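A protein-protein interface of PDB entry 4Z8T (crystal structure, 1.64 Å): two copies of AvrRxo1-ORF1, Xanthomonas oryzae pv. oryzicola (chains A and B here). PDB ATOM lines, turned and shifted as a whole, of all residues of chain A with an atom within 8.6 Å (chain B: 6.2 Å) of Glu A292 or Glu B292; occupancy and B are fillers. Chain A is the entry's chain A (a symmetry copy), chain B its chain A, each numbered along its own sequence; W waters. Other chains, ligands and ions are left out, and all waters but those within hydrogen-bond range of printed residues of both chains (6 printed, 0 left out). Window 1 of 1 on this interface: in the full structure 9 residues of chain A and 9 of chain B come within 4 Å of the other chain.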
ATOM      1  N   LYS A 287     -25.242  24.526  -3.674  1.00  0.00           N
ATOM      2  CA  LYS A 287     -25.432  24.911  -2.276  1.00  0.00           C
ATOM      3  C   LYS A 287     -24.108  24.876  -1.503  1.00  0.00           C
ATOM      4  O   LYS A 287     -23.376  23.881  -1.543  1.00  0.00           O
ATOM      5  CB  LYS A 287     -26.454  23.985  -1.610  1.00  0.00           C
ATOM      6  CG  LYS A 287     -26.709  24.282  -0.154  1.00  0.00           C
ATOM      7  CD  LYS A 287     -27.270  25.683   0.021  1.00  0.00           C
ATOM      8  CE  LYS A 287     -27.454  26.042   1.490  1.00  0.00           C
ATOM      9  NZ  LYS A 287     -26.158  26.166   2.215  1.00  0.00           N
ATOM     10  N   VAL A 288     -23.796  25.964  -0.802  1.00  0.00           N
ATOM     11  CA  VAL A 288     -22.532  26.050  -0.083  1.00  0.00           C
ATOM     12  C   VAL A 288     -22.623  25.492   1.331  1.00  0.00           C
ATOM     13  O   VAL A 288     -23.547  25.808   2.084  1.00  0.00           O
ATOM     14  CB  VAL A 288     -22.012  27.508  -0.046  1.00  0.00           C
ATOM     15  CG1 VAL A 288     -20.850  27.641   0.936  1.00  0.00           C
ATOM     16  CG2 VAL A 288     -21.582  27.932  -1.432  1.00  0.00           C
ATOM     17  N   ILE A 289     -21.657  24.654   1.688  1.00  0.00           N
ATOM     18  CA  ILE A 289     -21.565  24.153   3.048  1.00  0.00           C
ATOM     19  C   ILE A 289     -21.089  25.278   3.962  1.00  0.00           C
ATOM     20  O   ILE A 289     -19.886  25.576   4.013  1.00  0.00           O
ATOM     21  CB  ILE A 289     -20.594  22.973   3.127  1.00  0.00           C
ATOM     22  CG1 ILE A 289     -21.078  21.838   2.225  1.00  0.00           C
ATOM     23  CG2 ILE A 289     -20.444  22.480   4.560  1.00  0.00           C
ATOM     24  CD1 ILE A 289     -20.036  20.727   2.051  1.00  0.00           C
ATOM     25  N   ASP A 290     -22.032  25.905   4.662  1.00  0.00           N
ATOM     26  CA  ASP A 290     -21.706  26.986   5.601  1.00  0.00           C
ATOM     27  C   ASP A 290     -22.075  26.613   7.033  1.00  0.00           C
ATOM     28  O   ASP A 290     -22.569  25.512   7.278  1.00  0.00           O
ATOM     29  CB  ASP A 290     -22.363  28.318   5.191  1.00  0.00           C
ATOM     30  CG  ASP A 290     -23.889  28.237   5.083  1.00  0.00           C
ATOM     31  OD1 ASP A 290     -24.501  27.242   5.521  1.00  0.00           O
ATOM     32  OD2 ASP A 290     -24.500  29.202   4.566  1.00  0.00           O
ATOM     33  N   LYS A 291     -21.821  27.518   7.980  1.00  0.00           N
ATOM     34  CA  LYS A 291     -22.144  27.249   9.380  1.00  0.00           C
ATOM     35  C   LYS A 291     -23.612  26.866   9.534  1.00  0.00           C
ATOM     36  O   LYS A 291     -23.953  25.950  10.284  1.00  0.00           O
ATOM     37  CB  LYS A 291     -21.837  28.469  10.259  1.00  0.00           C
ATOM     38  CG  LYS A 291     -22.132  28.250  11.743  1.00  0.00           C
ATOM     39  CD  LYS A 291     -22.212  29.573  12.498  1.00  0.00           C
ATOM     40  CE  LYS A 291     -22.339  29.364  14.007  1.00  0.00           C
ATOM     41  NZ  LYS A 291     -23.569  28.637  14.407  1.00  0.00           N
ATOM     42  N   GLU A 292     -24.477  27.568   8.812  1.00  0.00           N
ATOM     43  CA  GLU A 292     -25.909  27.327   8.914  1.00  0.00           C
ATOM     44  C   GLU A 292     -26.264  25.909   8.489  1.00  0.00           C
ATOM     45  O   GLU A 292     -26.974  25.204   9.208  1.00  0.00           O
ATOM     46  CB  GLU A 292     -26.685  28.348   8.081  1.00  0.00           C
ATOM     47  CG  GLU A 292     -28.170  28.041   7.921  1.00  0.00           C
ATOM     48  CD  GLU A 292     -28.824  27.540   9.198  1.00  0.00           C
ATOM     49  OE1 GLU A 292     -28.588  28.123  10.284  1.00  0.00           O
ATOM     50  OE2 GLU A 292     -29.578  26.546   9.107  1.00  0.00           O
ATOM     51  N   LEU A 293     -25.758  25.498   7.331  1.00  0.00           N
ATOM     52  CA  LEU A 293     -26.017  24.153   6.808  1.00  0.00           C
ATOM     53  C   LEU A 293     -25.553  23.090   7.801  1.00  0.00           C
ATOM     54  O   LEU A 293     -26.282  22.136   8.081  1.00  0.00           O
ATOM     55  CB  LEU A 293     -25.344  23.964   5.440  1.00  0.00           C
ATOM     56  CG  LEU A 293     -25.517  22.625   4.701  1.00  0.00           C
ATOM     57  CD1 LEU A 293     -25.516  22.835   3.193  1.00  0.00           C
ATOM     58  CD2 LEU A 293     -24.430  21.619   5.062  1.00  0.00           C
ATOM     59  N   ILE A 294     -24.343  23.248   8.334  1.00  0.00           N
ATOM     60  CA  ILE A 294     -23.832  22.286   9.304  1.00  0.00           C
ATOM     61  C   ILE A 294     -24.722  22.263  10.547  1.00  0.00           C
ATOM     62  O   ILE A 294     -25.098  21.198  11.018  1.00  0.00           O
ATOM     63  CB  ILE A 294     -22.358  22.567   9.665  1.00  0.00           C
ATOM     64  CG1 ILE A 294     -21.496  22.483   8.396  1.00  0.00           C
ATOM     65  CG2 ILE A 294     -21.870  21.581  10.693  1.00  0.00           C
ATOM     66  CD1 ILE A 294     -20.052  22.928   8.588  1.00  0.00           C
ATOM     67  N   ASP A 295     -25.085  23.440  11.051  1.00  0.00           N
ATOM     68  CA  ASP A 295     -26.016  23.520  12.173  1.00  0.00           C
ATOM     69  C   ASP A 295     -27.375  22.917  11.828  1.00  0.00           C
ATOM     70  O   ASP A 295     -27.991  22.270  12.668  1.00  0.00           O
ATOM     71  CB  ASP A 295     -26.214  24.973  12.613  1.00  0.00           C
ATOM     72  CG  ASP A 295     -24.976  25.563  13.252  1.00  0.00           C
ATOM     73  OD1 ASP A 295     -24.035  24.794  13.565  1.00  0.00           O
ATOM     74  OD2 ASP A 295     -24.954  26.801  13.446  1.00  0.00           O
ATOM     75  N   ARG A 296     -27.842  23.145  10.603  1.00  0.00           N
ATOM     76  CA  ARG A 296     -29.139  22.618  10.177  1.00  0.00           C
ATOM     77  C   ARG A 296     -29.145  21.094  10.202  1.00  0.00           C
ATOM     78  O   ARG A 296     -30.092  20.487  10.699  1.00  0.00           O
ATOM     79  CB  ARG A 296     -29.515  23.117   8.781  1.00  0.00           C
ATOM     80  CG  ARG A 296     -30.799  22.487   8.238  1.00  0.00           C
ATOM     81  CD  ARG A 296     -31.285  23.159   6.969  1.00  0.00           C
ATOM     82  NE  ARG A 296     -30.283  23.170   5.904  1.00  0.00           N
ATOM     83  CZ  ARG A 296     -30.077  22.168   5.052  1.00  0.00           C
ATOM     84  NH1 ARG A 296     -30.791  21.054   5.142  1.00  0.00           N
ATOM     85  NH2 ARG A 296     -29.148  22.278   4.108  1.00  0.00           N
ATOM     86  N   LEU A 297     -28.082  20.480   9.682  1.00  0.00           N
ATOM     87  CA  LEU A 297     -27.963  19.021   9.711  1.00  0.00           C
ATOM     88  C   LEU A 297     -27.736  18.485  11.118  1.00  0.00           C
ATOM     89  O   LEU A 297     -28.289  17.447  11.490  1.00  0.00           O
ATOM     90  CB  LEU A 297     -26.857  18.544   8.770  1.00  0.00           C
ATOM     91  CG  LEU A 297     -27.143  18.788   7.287  1.00  0.00           C
ATOM     92  CD1 LEU A 297     -26.003  18.305   6.413  1.00  0.00           C
ATOM     93  CD2 LEU A 297     -28.430  18.109   6.875  1.00  0.00           C
ATOM     94  N   GLU A 298     -26.927  19.186  11.904  1.00  0.00           N
ATOM     95  CA  GLU A 298     -26.683  18.778  13.280  1.00  0.00           C
ATOM     96  C   GLU A 298     -27.954  18.820  14.128  1.00  0.00           C
ATOM     97  O   GLU A 298     -28.099  18.040  15.064  1.00  0.00           O
ATOM     98  CB  GLU A 298     -25.599  19.653  13.915  1.00  0.00           C
ATOM     99  CG  GLU A 298     -24.217  19.441  13.335  1.00  0.00           C
ATOM    100  CD  GLU A 298     -23.535  18.205  13.879  1.00  0.00           C
ATOM    101  OE1 GLU A 298     -23.239  18.179  15.095  1.00  0.00           O
ATOM    102  OE2 GLU A 298     -23.277  17.267  13.092  1.00  0.00           O
ATOM    103  N   ASN A 299     -28.869  19.733  13.798  1.00  0.00           N
ATOM    104  CA  ASN A 299     -30.105  19.909  14.568  1.00  0.00           C
ATOM    105  C   ASN A 299     -30.974  18.653  14.560  1.00  0.00           C
ATOM    106  O   ASN A 299     -31.775  18.438  15.474  1.00  0.00           O
ATOM    107  CB  ASN A 299     -30.904  21.099  14.020  1.00  0.00           C
ATOM    108  CG  ASN A 299     -31.992  21.565  14.971  1.00  0.00           C
ATOM    109  OD1 ASN A 299     -31.770  21.667  16.180  1.00  0.00           O
ATOM    110  ND2 ASN A 299     -33.174  21.854  14.430  1.00  0.00           N
ATOM    111  N   ASN A 300     -30.815  17.826  13.526  1.00  0.00           N
ATOM    112  CA  ASN A 300     -31.605  16.596  13.399  1.00  0.00           C
ATOM    113  C   ASN A 300     -30.796  15.321  13.603  1.00  0.00           C
ATOM    114  O   ASN A 300     -31.199  14.225  13.197  1.00  0.00           O
ATOM    115  CB  ASN A 300     -32.352  16.555  12.060  1.00  0.00           C
ATOM    116  CG  ASN A 300     -33.478  17.568  11.990  1.00  0.00           C
ATOM    117  OD1 ASN A 300     -33.526  18.402  11.086  1.00  0.00           O
ATOM    118  ND2 ASN A 300     -34.387  17.499  12.946  1.00  0.00           N
ATOM    119  N   LEU A 314     -18.108  17.681   7.367  1.00  0.00           N
ATOM    120  CA  LEU A 314     -18.588  18.889   6.707  1.00  0.00           C
ATOM    121  C   LEU A 314     -17.614  20.047   6.880  1.00  0.00           C
ATOM    122  O   LEU A 314     -17.378  20.798   5.941  1.00  0.00           O
ATOM    123  CB  LEU A 314     -19.963  19.287   7.240  1.00  0.00           C
ATOM    124  CG  LEU A 314     -21.122  18.359   6.866  1.00  0.00           C
ATOM    125  CD1 LEU A 314     -22.391  18.701   7.632  1.00  0.00           C
ATOM    126  CD2 LEU A 314     -21.373  18.464   5.376  1.00  0.00           C
ATOM    127  N   GLU A 315     -17.055  20.188   8.077  1.00  0.00           N
ATOM    128  CA  GLU A 315     -16.164  21.318   8.357  1.00  0.00           C
ATOM    129  C   GLU A 315     -14.930  21.295   7.459  1.00  0.00           C
ATOM    130  O   GLU A 315     -14.412  22.353   7.080  1.00  0.00           O
ATOM    131  CB  GLU A 315     -15.759  21.355   9.838  1.00  0.00           C
ATOM    132  CG  GLU A 315     -16.898  21.645  10.817  1.00  0.00           C
ATOM    133  CD  GLU A 315     -17.301  23.114  10.868  1.00  0.00           C
ATOM    134  OE1 GLU A 315     -16.685  23.935  10.152  1.00  0.00           O
ATOM    135  OE2 GLU A 315     -18.232  23.449  11.636  1.00  0.00           O
ATOM    136  N   SER A 318     -15.920  23.248   4.521  1.00  0.00           N
ATOM    137  CA  SER A 318     -16.638  24.491   4.783  1.00  0.00           C
ATOM    138  C   SER A 318     -16.314  25.523   3.696  1.00  0.00           C
ATOM    139  O   SER A 318     -15.153  25.668   3.303  1.00  0.00           O
ATOM    140  CB  SER A 318     -16.264  25.032   6.165  1.00  0.00           C
ATOM    141  OG  SER A 318     -17.278  25.885   6.670  1.00  0.00           O
ATOM    142  N   ASP B 290     -37.268  27.119  17.135  1.00  0.00           N
ATOM    143  CA  ASP B 290     -36.077  26.898  17.965  1.00  0.00           C
ATOM    144  C   ASP B 290     -34.896  27.732  17.480  1.00  0.00           C
ATOM    145  O   ASP B 290     -35.022  28.481  16.511  1.00  0.00           O
ATOM    146  CB  ASP B 290     -35.703  25.405  18.044  1.00  0.00           C
ATOM    147  CG  ASP B 290     -35.444  24.769  16.675  1.00  0.00           C
ATOM    148  OD1 ASP B 290     -35.328  25.482  15.659  1.00  0.00           O
ATOM    149  OD2 ASP B 290     -35.330  23.521  16.612  1.00  0.00           O
ATOM    150  N   LYS B 291     -33.754  27.618  18.161  1.00  0.00           N
ATOM    151  CA  LYS B 291     -32.568  28.376  17.768  1.00  0.00           C
ATOM    152  C   LYS B 291     -32.222  28.123  16.305  1.00  0.00           C
ATOM    153  O   LYS B 291     -31.870  29.045  15.567  1.00  0.00           O
ATOM    154  CB  LYS B 291     -31.365  28.013  18.649  1.00  0.00           C
ATOM    155  CG  LYS B 291     -30.092  28.786  18.307  1.00  0.00           C
ATOM    156  CD  LYS B 291     -28.856  28.119  18.901  1.00  0.00           C
ATOM    157  CE  LYS B 291     -27.599  28.968  18.710  1.00  0.00           C
ATOM    158  NZ  LYS B 291     -27.245  29.198  17.286  1.00  0.00           N
ATOM    159  N   GLU B 292     -32.334  26.868  15.888  1.00  0.00           N
ATOM    160  CA  GLU B 292     -31.982  26.495  14.525  1.00  0.00           C
ATOM    161  C   GLU B 292     -32.861  27.214  13.511  1.00  0.00           C
ATOM    162  O   GLU B 292     -32.353  27.804  12.557  1.00  0.00           O
ATOM    163  CB  GLU B 292     -32.078  24.981  14.342  1.00  0.00           C
ATOM    164  CG  GLU B 292     -31.970  24.507  12.896  1.00  0.00           C
ATOM    165  CD  GLU B 292     -30.904  25.241  12.099  1.00  0.00           C
ATOM    166  OE1 GLU B 292     -29.772  25.433  12.607  1.00  0.00           O
ATOM    167  OE2 GLU B 292     -31.212  25.633  10.952  1.00  0.00           O
ATOM    168  N   LEU B 293     -34.171  27.169  13.732  1.00  0.00           N
ATOM    169  CA  LEU B 293     -35.128  27.824  12.836  1.00  0.00           C
ATOM    170  C   LEU B 293     -34.833  29.319  12.729  1.00  0.00           C
ATOM    171  O   LEU B 293     -34.807  29.874  11.629  1.00  0.00           O
ATOM    172  CB  LEU B 293     -36.569  27.578  13.308  1.00  0.00           C
ATOM    173  CG  LEU B 293     -37.735  28.158  12.486  1.00  0.00           C
ATOM    174  CD1 LEU B 293     -38.958  27.255  12.568  1.00  0.00           C
ATOM    175  CD2 LEU B 293     -38.122  29.561  12.940  1.00  0.00           C
ATOM    176  N   ILE B 294     -34.610  29.973  13.867  1.00  0.00           N
ATOM    177  CA  ILE B 294     -34.303  31.398  13.852  1.00  0.00           C
ATOM    178  C   ILE B 294     -33.005  31.653  13.084  1.00  0.00           C
ATOM    179  O   ILE B 294     -32.950  32.536  12.238  1.00  0.00           O
ATOM    180  CB  ILE B 294     -34.244  31.987  15.278  1.00  0.00           C
ATOM    181  CG1 ILE B 294     -35.603  31.788  15.967  1.00  0.00           C
ATOM    182  CG2 ILE B 294     -33.891  33.449  15.231  1.00  0.00           C
ATOM    183  CD1 ILE B 294     -35.615  32.156  17.446  1.00  0.00           C
ATOM    184  N   ASP B 295     -31.976  30.854  13.356  1.00  0.00           N
ATOM    185  CA  ASP B 295     -30.730  30.952  12.602  1.00  0.00           C
ATOM    186  C   ASP B 295     -30.939  30.666  11.118  1.00  0.00           C
ATOM    187  O   ASP B 295     -30.325  31.311  10.275  1.00  0.00           O
ATOM    188  CB  ASP B 295     -29.682  29.981  13.153  1.00  0.00           C
ATOM    189  CG  ASP B 295     -29.192  30.370  14.530  1.00  0.00           C
ATOM    190  OD1 ASP B 295     -29.485  31.507  14.974  1.00  0.00           O
ATOM    191  OD2 ASP B 295     -28.506  29.534  15.162  1.00  0.00           O
ATOM    192  N   ARG B 296     -31.789  29.691  10.806  1.00  0.00           N
ATOM    193  CA  ARG B 296     -32.054  29.333   9.412  1.00  0.00           C
ATOM    194  C   ARG B 296     -32.674  30.502   8.655  1.00  0.00           C
ATOM    195  O   ARG B 296     -32.258  30.808   7.539  1.00  0.00           O
ATOM    196  CB  ARG B 296     -32.961  28.106   9.310  1.00  0.00           C
ATOM    197  CG  ARG B 296     -33.374  27.775   7.875  1.00  0.00           C
ATOM    198  CD  ARG B 296     -34.070  26.433   7.765  1.00  0.00           C
ATOM    199  NE  ARG B 296     -35.245  26.322   8.627  1.00  0.00           N
ATOM    200  CZ  ARG B 296     -36.463  26.751   8.299  1.00  0.00           C
ATOM    201  NH1 ARG B 296     -36.674  27.341   7.130  1.00  0.00           N
ATOM    202  NH2 ARG B 296     -37.474  26.594   9.148  1.00  0.00           N
ATOM    203  N   LEU B 297     -33.657  31.161   9.270  1.00  0.00           N
ATOM    204  CA  LEU B 297     -34.279  32.335   8.654  1.00  0.00           C
ATOM    205  C   LEU B 297     -33.339  33.532   8.607  1.00  0.00           C
ATOM    206  O   LEU B 297     -33.314  34.271   7.620  1.00  0.00           O
ATOM    207  CB  LEU B 297     -35.580  32.701   9.367  1.00  0.00           C
ATOM    208  CG  LEU B 297     -36.694  31.663   9.217  1.00  0.00           C
ATOM    209  CD1 LEU B 297     -37.949  32.082   9.958  1.00  0.00           C
ATOM    210  CD2 LEU B 297     -37.012  31.432   7.757  1.00  0.00           C
ATOM    211  N   ASN B 299     -30.192  33.426   8.276  1.00  0.00           N
ATOM    212  CA  ASN B 299     -29.134  33.150   7.300  1.00  0.00           C
ATOM    213  C   ASN B 299     -29.451  33.734   5.924  1.00  0.00           C
ATOM    214  O   ASN B 299     -28.543  34.009   5.134  1.00  0.00           O
ATOM    215  CB  ASN B 299     -28.904  31.637   7.184  1.00  0.00           C
ATOM    216  CG  ASN B 299     -27.603  31.292   6.481  1.00  0.00           C
ATOM    217  OD1 ASN B 299     -26.565  31.904   6.741  1.00  0.00           O
ATOM    218  ND2 ASN B 299     -27.651  30.306   5.587  1.00  0.00           N
HETATM  219  O   HOH W   1     -34.453  21.957  18.303  1.00  0.00           O
HETATM  220  O   HOH W   2     -31.974  24.455  17.517  1.00  0.00           O
HETATM  221  O   HOH W   3     -26.836  27.290   4.390  1.00  0.00           O
HETATM  222  O   HOH W   4     -23.914  31.596   4.582  1.00  0.00           O
HETATM  223  O   HOH W   5     -35.698  23.901  13.634  1.00  0.00           O
HETATM  224  O   HOH W   6     -24.172  30.358   7.959  1.00  0.00           O
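The side-chain carboxylate (OD2) of Asp B290 is in hydrogen-bond range of the side-chain amide nitrogen (ND2) of Asn A299 (3.5 Å). The side-chain carboxylate (OE2) of Glu A292 sits close to the side-chain carboxylate (OE2) of Glu B292 (2.6 Å). The side-chain carboxylate (OD2) of Asp A290 sits at hydrogen-bond distance from the side-chain amide nitrogen (ND2) of Asn B299, 3.5 Å away.
Water W1 bridges OD2 of Asp B290 (2.5 Å) and OD1 of Asn A299 (3.4 Å). Water W4 lies within hydrogen-bond range of OD2 of Asp A290 and OD1 of Asn B299. Water W3 lies within hydrogen-bond range of NZ of Lys A287 (2.5 Å), OD1 of Asp A290 (2.6 Å) and ND2 of Asn B299 (3.3 Å). Water W5 bridges the side-chain carboxylate (OD1) of Asp B290 (2.6 Å) and the side-chain amide nitrogen (ND2) of Asn A299 (3.3 Å). Water W2 lies within hydrogen-bond range of the backbone NH of Glu B292 (2.9 Å) and the side-chain amide oxygen of Asn A299 (3.1 Å). Water W6 bridges the backbone NH (N) of Glu A292 and the side-chain amide oxygen (OD1) of Asn B299.
Asp A290 touches Asn B299, and with the chains exchanged Asn A299 touches Asp B290. Glu B292 touches its own counterpart, Glu A292. Glu A292 touches Asp B295, and with the chains exchanged Asp A295 touches Glu B292. Glu A292 touches Arg B296, and with the chains exchanged Arg A296 touches Glu B292. Positions printed for both chains: 290, 291, 292, 293, 294, 295, 296, 297 and 299. Of the 9 pairs that touch across the chains among the printed residues, 9 have their exchanged pair printed and touching as well.
Printed residues of chain B that touch a printed residue of chain A: Asp B290, Glu B292, Asp B295, Arg B296 and Asn B299. Along chain B the printed residues that touch a printed residue of chain A span positions 290 to 299. Among the printed residues, 9 pairs touch across the chains.
OE1 of Glu A292 touches C of Asp B295, 3.6 Å away. Glu A292 touches Arg B296. CG of Glu A292 touches ND2 of Asn B299 (3.3 Å). Asp A295 touches Glu B292 (C to OE1, 3.6 Å). Glu B292 touches Arg A296 (OE1 to N, 3.6 Å). Glu B292 touches Asn A299.
Lys A287 touches none of the printed residues of chain B. Printed residues of chain B within 4 Å of Asp A290: Asn B299 (3.5 Å). Of chain B, only Glu B292 (2.6 Å), Asp B295 (3.6 Å), Arg B296 (3.6 Å) and Asn B299 (3.3 Å) come within 4 Å of Glu A292. Of the printed residues of chain B, Asn A299 touches Asp B290 (3.5 Å) and Glu B292 (3.3 Å). Glu B292 touches just these residues of chain A: Glu A292, Asp A295, Arg A296 and Asn A299. Leu B293 touches none of the printed residues of chain A. Of the printed residues of chain A, Asp B295 touches Glu A292 (3.6 Å). The nearest residue of chain B that does not touch Glu A292 is Leu B297 (6.0 Å).
The backbone NH (N) of Glu B292 sits close to the side-chain carboxylate (OD1) of Asp B290 (3.3 Å). The side-chain carboxylate (OD1) of Asp B290 is in hydrogen-bond range of the backbone NH (N) of Leu B293. The side-chain amino group (NZ) of Lys B291 is in salt-bridge range of the side-chain carboxylate (OD2) of Asp B295 (2.5 Å). The side-chain carboxylate of Asp A290 is in salt-bridge range of the side-chain amino group of Lys A287 (3.9 Å). The side-chain carboxylate of Asp A290 sits at hydrogen-bond distance from the backbone NH of Leu A293 (2.8 Å). The side-chain amino group (NZ) of Lys A291 lies within salt-bridge range of the side-chain carboxylate (OD2) of Asp A295, at 2.5 Å.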
